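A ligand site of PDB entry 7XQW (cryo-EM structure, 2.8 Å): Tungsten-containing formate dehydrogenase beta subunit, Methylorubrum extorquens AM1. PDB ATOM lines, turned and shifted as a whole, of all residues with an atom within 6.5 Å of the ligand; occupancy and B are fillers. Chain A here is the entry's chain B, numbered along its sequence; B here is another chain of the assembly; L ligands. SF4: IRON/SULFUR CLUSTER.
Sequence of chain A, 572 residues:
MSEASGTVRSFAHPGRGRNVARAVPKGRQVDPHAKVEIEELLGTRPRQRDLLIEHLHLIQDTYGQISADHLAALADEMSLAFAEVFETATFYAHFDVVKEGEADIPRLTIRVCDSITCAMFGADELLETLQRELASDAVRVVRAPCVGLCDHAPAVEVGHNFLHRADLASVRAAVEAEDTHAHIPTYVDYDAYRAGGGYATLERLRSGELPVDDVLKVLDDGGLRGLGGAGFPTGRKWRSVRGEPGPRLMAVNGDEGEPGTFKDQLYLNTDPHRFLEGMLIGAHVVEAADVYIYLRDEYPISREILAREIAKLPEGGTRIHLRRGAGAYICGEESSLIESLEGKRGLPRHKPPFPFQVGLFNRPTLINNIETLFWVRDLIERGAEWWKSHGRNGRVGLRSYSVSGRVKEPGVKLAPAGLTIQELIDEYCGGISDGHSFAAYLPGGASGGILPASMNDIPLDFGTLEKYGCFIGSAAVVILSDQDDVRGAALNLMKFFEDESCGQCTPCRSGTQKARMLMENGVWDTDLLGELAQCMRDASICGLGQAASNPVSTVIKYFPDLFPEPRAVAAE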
ATOM      1  N   ILE A 330      19.547  25.672  10.743  1.00  0.00           N
ATOM      2  CA  ILE A 330      18.713  26.849  10.919  1.00  0.00           C
ATOM      3  C   ILE A 330      19.376  27.888  11.818  1.00  0.00           C
ATOM      4  O   ILE A 330      19.050  29.069  11.741  1.00  0.00           O
ATOM      5  CB  ILE A 330      17.334  26.448  11.466  1.00  0.00           C
ATOM      6  CG1 ILE A 330      16.368  27.632  11.464  1.00  0.00           C
ATOM      7  CG2 ILE A 330      17.475  25.897  12.874  1.00  0.00           C
ATOM      8  CD1 ILE A 330      16.234  28.324  10.126  1.00  0.00           C
ATOM      9  N   SER A 336      17.557  32.887  14.507  1.00  0.00           N
ATOM     10  CA  SER A 336      17.846  31.565  15.069  1.00  0.00           C
ATOM     11  C   SER A 336      19.170  31.562  15.819  1.00  0.00           C
ATOM     12  O   SER A 336      19.272  30.967  16.892  1.00  0.00           O
ATOM     13  CB  SER A 336      17.870  30.531  13.945  1.00  0.00           C
ATOM     14  OG  SER A 336      16.602  30.418  13.329  1.00  0.00           O
ATOM     15  N   LEU A 347      14.867  28.579  17.076  1.00  0.00           N
ATOM     16  CA  LEU A 347      13.720  28.937  16.264  1.00  0.00           C
ATOM     17  C   LEU A 347      13.828  30.401  15.840  1.00  0.00           C
ATOM     18  O   LEU A 347      14.018  31.269  16.694  1.00  0.00           O
ATOM     19  CB  LEU A 347      12.419  28.724  17.030  1.00  0.00           C
ATOM     20  CG  LEU A 347      11.780  27.336  16.972  1.00  0.00           C
ATOM     21  CD1 LEU A 347      12.604  26.327  17.747  1.00  0.00           C
ATOM     22  CD2 LEU A 347      10.370  27.391  17.509  1.00  0.00           C
ATOM     23  N   PRO A 348      13.712  30.714  14.554  1.00  0.00           N
ATOM     24  CA  PRO A 348      13.755  32.117  14.143  1.00  0.00           C
ATOM     25  C   PRO A 348      12.635  32.912  14.793  1.00  0.00           C
ATOM     26  O   PRO A 348      11.725  32.375  15.435  1.00  0.00           O
ATOM     27  CB  PRO A 348      13.609  32.052  12.618  1.00  0.00           C
ATOM     28  CG  PRO A 348      13.001  30.752  12.351  1.00  0.00           C
ATOM     29  CD  PRO A 348      13.547  29.829  13.386  1.00  0.00           C
ATOM     30  N   GLU A 500      16.293  19.736   8.074  1.00  0.00           N
ATOM     31  CA  GLU A 500      16.870  20.905   8.707  1.00  0.00           C
ATOM     32  C   GLU A 500      15.856  21.954   9.120  1.00  0.00           C
ATOM     33  O   GLU A 500      16.193  22.855   9.895  1.00  0.00           O
ATOM     34  CB  GLU A 500      17.919  21.544   7.774  1.00  0.00           C
ATOM     35  CG  GLU A 500      19.219  20.760   7.729  1.00  0.00           C
ATOM     36  CD  GLU A 500      19.866  20.610   9.087  1.00  0.00           C
ATOM     37  OE1 GLU A 500      19.317  21.140  10.072  1.00  0.00           O
ATOM     38  OE2 GLU A 500      20.923  19.949   9.179  1.00  0.00           O
ATOM     39  N   SER A 501      14.620  21.872   8.626  1.00  0.00           N
ATOM     40  CA  SER A 501      13.581  22.794   9.079  1.00  0.00           C
ATOM     41  C   SER A 501      13.416  22.692  10.588  1.00  0.00           C
ATOM     42  O   SER A 501      13.348  21.586  11.136  1.00  0.00           O
ATOM     43  CB  SER A 501      12.273  22.494   8.369  1.00  0.00           C
ATOM     44  OG  SER A 501      11.270  23.435   8.714  1.00  0.00           O
ATOM     45  N   CYS A 502      13.340  23.837  11.262  1.00  0.00           N
ATOM     46  CA  CYS A 502      13.139  23.826  12.711  1.00  0.00           C
ATOM     47  C   CYS A 502      11.742  23.355  13.097  1.00  0.00           C
ATOM     48  O   CYS A 502      11.511  23.082  14.273  1.00  0.00           O
ATOM     49  CB  CYS A 502      13.401  25.218  13.287  1.00  0.00           C
ATOM     50  SG  CYS A 502      12.012  26.353  13.229  1.00  0.00           S
ATOM     51  N   GLY A 503      10.834  23.249  12.135  1.00  0.00           N
ATOM     52  CA  GLY A 503       9.495  22.757  12.401  1.00  0.00           C
ATOM     53  C   GLY A 503       8.640  23.674  13.254  1.00  0.00           C
ATOM     54  O   GLY A 503       7.875  23.190  14.097  1.00  0.00           O
ATOM     55  N   GLN A 504       8.738  24.981  13.039  1.00  0.00           N
ATOM     56  CA  GLN A 504       7.930  25.939  13.766  1.00  0.00           C
ATOM     57  C   GLN A 504       6.622  26.248  13.048  1.00  0.00           C
ATOM     58  O   GLN A 504       5.549  26.100  13.633  1.00  0.00           O
ATOM     59  CB  GLN A 504       8.719  27.235  14.002  1.00  0.00           C
ATOM     60  CG  GLN A 504       7.940  28.303  14.740  1.00  0.00           C
ATOM     61  CD  GLN A 504       8.793  29.494  15.128  1.00  0.00           C
ATOM     62  OE1 GLN A 504      10.013  29.479  14.973  1.00  0.00           O
ATOM     63  NE2 GLN A 504       8.157  30.531  15.661  1.00  0.00           N
ATOM     64  N   CYS A 505       6.695  26.676  11.800  1.00  0.00           N
ATOM     65  CA  CYS A 505       5.512  27.028  11.024  1.00  0.00           C
ATOM     66  C   CYS A 505       5.087  25.846  10.155  1.00  0.00           C
ATOM     67  O   CYS A 505       5.821  24.878   9.950  1.00  0.00           O
ATOM     68  CB  CYS A 505       5.766  28.265  10.170  1.00  0.00           C
ATOM     69  SG  CYS A 505       7.099  28.137   8.965  1.00  0.00           S
ATOM     70  N   THR A 506       3.863  25.939   9.649  1.00  0.00           N
ATOM     71  CA  THR A 506       3.252  24.847   8.908  1.00  0.00           C
ATOM     72  C   THR A 506       3.828  24.728   7.500  1.00  0.00           C
ATOM     73  O   THR A 506       4.231  23.630   7.095  1.00  0.00           O
ATOM     74  CB  THR A 506       1.736  25.024   8.822  1.00  0.00           C
ATOM     75  OG1 THR A 506       1.151  24.714  10.091  1.00  0.00           O
ATOM     76  CG2 THR A 506       1.137  24.142   7.740  1.00  0.00           C
ATOM     77  N   PRO A 507       3.881  25.812   6.720  1.00  0.00           N
ATOM     78  CA  PRO A 507       4.315  25.663   5.321  1.00  0.00           C
ATOM     79  C   PRO A 507       5.651  24.974   5.193  1.00  0.00           C
ATOM     80  O   PRO A 507       5.808  24.074   4.363  1.00  0.00           O
ATOM     81  CB  PRO A 507       4.345  27.099   4.816  1.00  0.00           C
ATOM     82  CG  PRO A 507       3.412  27.833   5.682  1.00  0.00           C
ATOM     83  CD  PRO A 507       3.544  27.213   7.032  1.00  0.00           C
ATOM     84  N   CYS A 508       6.623  25.315   6.035  1.00  0.00           N
ATOM     85  CA  CYS A 508       7.918  24.651   5.977  1.00  0.00           C
ATOM     86  C   CYS A 508       7.857  23.255   6.583  1.00  0.00           C
ATOM     87  O   CYS A 508       8.111  22.265   5.904  1.00  0.00           O
ATOM     88  CB  CYS A 508       8.976  25.514   6.659  1.00  0.00           C
ATOM     89  SG  CYS A 508      10.611  24.762   6.790  1.00  0.00           S
ATOM     90  N   ARG A 509       7.466  23.167   7.859  1.00  0.00           N
ATOM     91  CA  ARG A 509       7.497  21.895   8.571  1.00  0.00           C
ATOM     92  C   ARG A 509       6.795  20.792   7.790  1.00  0.00           C
ATOM     93  O   ARG A 509       7.341  19.710   7.584  1.00  0.00           O
ATOM     94  CB  ARG A 509       6.858  22.054   9.948  1.00  0.00           C
ATOM     95  CG  ARG A 509       6.972  20.821  10.841  1.00  0.00           C
ATOM     96  CD  ARG A 509       5.752  20.642  11.738  1.00  0.00           C
ATOM     97  NE  ARG A 509       5.196  21.911  12.187  1.00  0.00           N
ATOM     98  CZ  ARG A 509       3.963  22.335  11.940  1.00  0.00           C
ATOM     99  NH1 ARG A 509       3.109  21.636  11.209  1.00  0.00           N
ATOM    100  NH2 ARG A 509       3.571  23.503  12.440  1.00  0.00           N
ATOM    101  N   THR A 512       7.876  20.710   3.446  1.00  0.00           N
ATOM    102  CA  THR A 512       9.100  19.988   3.091  1.00  0.00           C
ATOM    103  C   THR A 512       8.850  18.485   3.060  1.00  0.00           C
ATOM    104  O   THR A 512       9.261  17.800   2.120  1.00  0.00           O
ATOM    105  CB  THR A 512      10.213  20.339   4.081  1.00  0.00           C
ATOM    106  OG1 THR A 512       9.744  20.154   5.422  1.00  0.00           O
ATOM    107  CG2 THR A 512      10.657  21.779   3.905  1.00  0.00           C
ATOM    108  N   SER A 540       5.843  31.088   4.642  1.00  0.00           N
ATOM    109  CA  SER A 540       6.886  30.618   5.549  1.00  0.00           C
ATOM    110  C   SER A 540       7.392  31.761   6.425  1.00  0.00           C
ATOM    111  O   SER A 540       7.416  32.925   6.019  1.00  0.00           O
ATOM    112  CB  SER A 540       8.042  30.016   4.758  1.00  0.00           C
ATOM    113  OG  SER A 540       7.635  28.812   4.121  1.00  0.00           O
ATOM    114  N   ILE A 541       7.790  31.414   7.651  1.00  0.00           N
ATOM    115  CA  ILE A 541       8.258  32.421   8.595  1.00  0.00           C
ATOM    116  C   ILE A 541       9.608  32.987   8.142  1.00  0.00           C
ATOM    117  O   ILE A 541       9.725  34.167   7.827  1.00  0.00           O
ATOM    118  CB  ILE A 541       8.345  31.835  10.012  1.00  0.00           C
ATOM    119  CG1 ILE A 541       6.957  31.785  10.660  1.00  0.00           C
ATOM    120  CG2 ILE A 541       9.297  32.654  10.865  1.00  0.00           C
ATOM    121  CD1 ILE A 541       6.917  30.966  11.933  1.00  0.00           C
ATOM    122  N   CYS A 542      10.623  32.137   8.103  1.00  0.00           N
ATOM    123  CA  CYS A 542      11.983  32.559   7.837  1.00  0.00           C
ATOM    124  C   CYS A 542      12.370  32.236   6.399  1.00  0.00           C
ATOM    125  O   CYS A 542      11.535  31.841   5.580  1.00  0.00           O
ATOM    126  CB  CYS A 542      12.950  31.907   8.832  1.00  0.00           C
ATOM    127  SG  CYS A 542      13.333  30.189   8.471  1.00  0.00           S
ATOM    128  N   GLY A 543      13.656  32.419   6.075  1.00  0.00           N
ATOM    129  CA  GLY A 543      14.129  32.166   4.726  1.00  0.00           C
ATOM    130  C   GLY A 543      14.410  30.717   4.421  1.00  0.00           C
ATOM    131  O   GLY A 543      14.506  30.358   3.243  1.00  0.00           O
ATOM    132  N   LEU A 544      14.546  29.867   5.438  1.00  0.00           N
ATOM    133  CA  LEU A 544      14.768  28.443   5.190  1.00  0.00           C
ATOM    134  C   LEU A 544      13.609  27.846   4.406  1.00  0.00           C
ATOM    135  O   LEU A 544      13.806  27.125   3.425  1.00  0.00           O
ATOM    136  CB  LEU A 544      14.957  27.705   6.517  1.00  0.00           C
ATOM    137  CG  LEU A 544      15.563  26.297   6.430  1.00  0.00           C
ATOM    138  CD1 LEU A 544      16.286  25.953   7.715  1.00  0.00           C
ATOM    139  CD2 LEU A 544      14.495  25.261   6.128  1.00  0.00           C
ATOM    140  N   GLY A 545      12.377  28.147   4.830  1.00  0.00           N
ATOM    141  CA  GLY A 545      11.214  27.640   4.119  1.00  0.00           C
ATOM    142  C   GLY A 545      10.878  28.429   2.886  1.00  0.00           C
ATOM    143  O   GLY A 545      10.326  27.875   1.931  1.00  0.00           O
ATOM    144  N   GLN A 546      11.208  29.726   2.871  1.00  0.00           N
ATOM    145  CA  GLN A 546      10.957  30.547   1.686  1.00  0.00           C
ATOM    146  C   GLN A 546      11.834  30.150   0.508  1.00  0.00           C
ATOM    147  O   GLN A 546      11.562  30.577  -0.615  1.00  0.00           O
ATOM    148  CB  GLN A 546      11.153  32.016   2.022  1.00  0.00           C
ATOM    149  CG  GLN A 546      10.110  32.583   2.966  1.00  0.00           C
ATOM    150  CD  GLN A 546      10.438  33.990   3.417  1.00  0.00           C
ATOM    151  OE1 GLN A 546      11.485  34.531   3.092  1.00  0.00           O
ATOM    152  NE2 GLN A 546       9.522  34.593   4.169  1.00  0.00           N
ATOM    153  N   ALA B 238      11.742  19.998  13.022  1.00  0.00           N
ATOM    154  CA  ALA B 238      11.054  19.645  11.781  1.00  0.00           C
ATOM    155  C   ALA B 238       9.737  18.940  12.070  1.00  0.00           C
ATOM    156  O   ALA B 238       9.159  19.115  13.148  1.00  0.00           O
ATOM    157  CB  ALA B 238      11.952  18.766  10.911  1.00  0.00           C
HETATM  158 FE1  SF4 L   1      11.851  28.685   9.259  1.00  0.00          FE
HETATM  159 FE2  SF4 L   1      11.061  26.174   8.502  1.00  0.00          FE
HETATM  160 FE3  SF4 L   1       9.257  27.899   9.600  1.00  0.00          FE
HETATM  161 FE4  SF4 L   1      11.227  26.823  11.158  1.00  0.00          FE
HETATM  162  S1  SF4 L   1       9.536  25.698  10.132  1.00  0.00           S
HETATM  163  S2  SF4 L   1      10.552  29.000  11.117  1.00  0.00           S
HETATM  164  S3  SF4 L   1      12.949  26.722   9.665  1.00  0.00           S
HETATM  165  S4  SF4 L   1      10.365  28.162   7.634  1.00  0.00           S
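A sulfur (S3) of the ligand lies close to the backbone NH (N) of Cys 502, at 3.3 Å.
N of Gly 545 lies close to S4 of the ligand.
The backbone NH (N) of Gly 503 sits close to a sulfur (S1) of the ligand (3.4 Å).
S1 of the ligand sits close to N of Cys 505.
The side-chain sulfur of Cys 505 is bound to an iron atom (FE3) of the ligand (2.3 Å).
S1 of the ligand sits close to OG of Ser 501 (3.2 Å).
An iron atom (FE4) of the ligand is bound by the side-chain sulfur of Cys 502 (2.3 Å).
N of Gln 504 lies close to S1 of the ligand (3.1 Å).
An iron atom (FE2) of the ligand is bound by the side-chain sulfur (SG) of Cys 508.
FE1 of the ligand is bound by SG of Cys 542 (2.3 Å).
N of Gln 504 lies close to SG of Cys 502, at 3.6 Å.
OG1 of Thr 512 sits at hydrogen-bond distance from O of Arg 509 (3.3 Å).
The side-chain sulfur (SG) of Cys 508 lies close to the side-chain hydroxyl (OG) of Ser 501.
N of Leu 544 sits close to SG of Cys 542.
The backbone NH (N) of Ile 541 lies close to the side-chain sulfur (SG) of Cys 505 (3.6 Å).
O of Cys 502 lies within hydrogen-bond range of N of Ala 238 of chain B (3.3 Å).
O of Ile 330 sits close to OG of Ser 336, at 3.2 Å.
The guanidinium group (NH2) of Arg 509 is in hydrogen-bond range of the backbone carbonyl oxygen (O) of Gln 504 (3.5 Å).
Merely in contact with the ligand: Pro 348 (3.3 Å), Ile 330 (3.7 Å), Ile 541 (3.8 Å), Leu 544 (3.9 Å) and Arg 509 (3.98 Å).
Hydrophobic or aromatic side chains within 4 Å of the ligand: Ile 330, Pro 348, Ile 541 and Leu 544.
13 residues have an atom within 4 Å of the ligand: Ile 330, Pro 348, Ser 501, Cys 502, Gly 503, Gln 504, Cys 505, Cys 508, Arg 509, Ile 541, Cys 542, Leu 544 and Gly 545.
Along chain A the residues within 4 Å of the ligand span positions 330 to 545.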
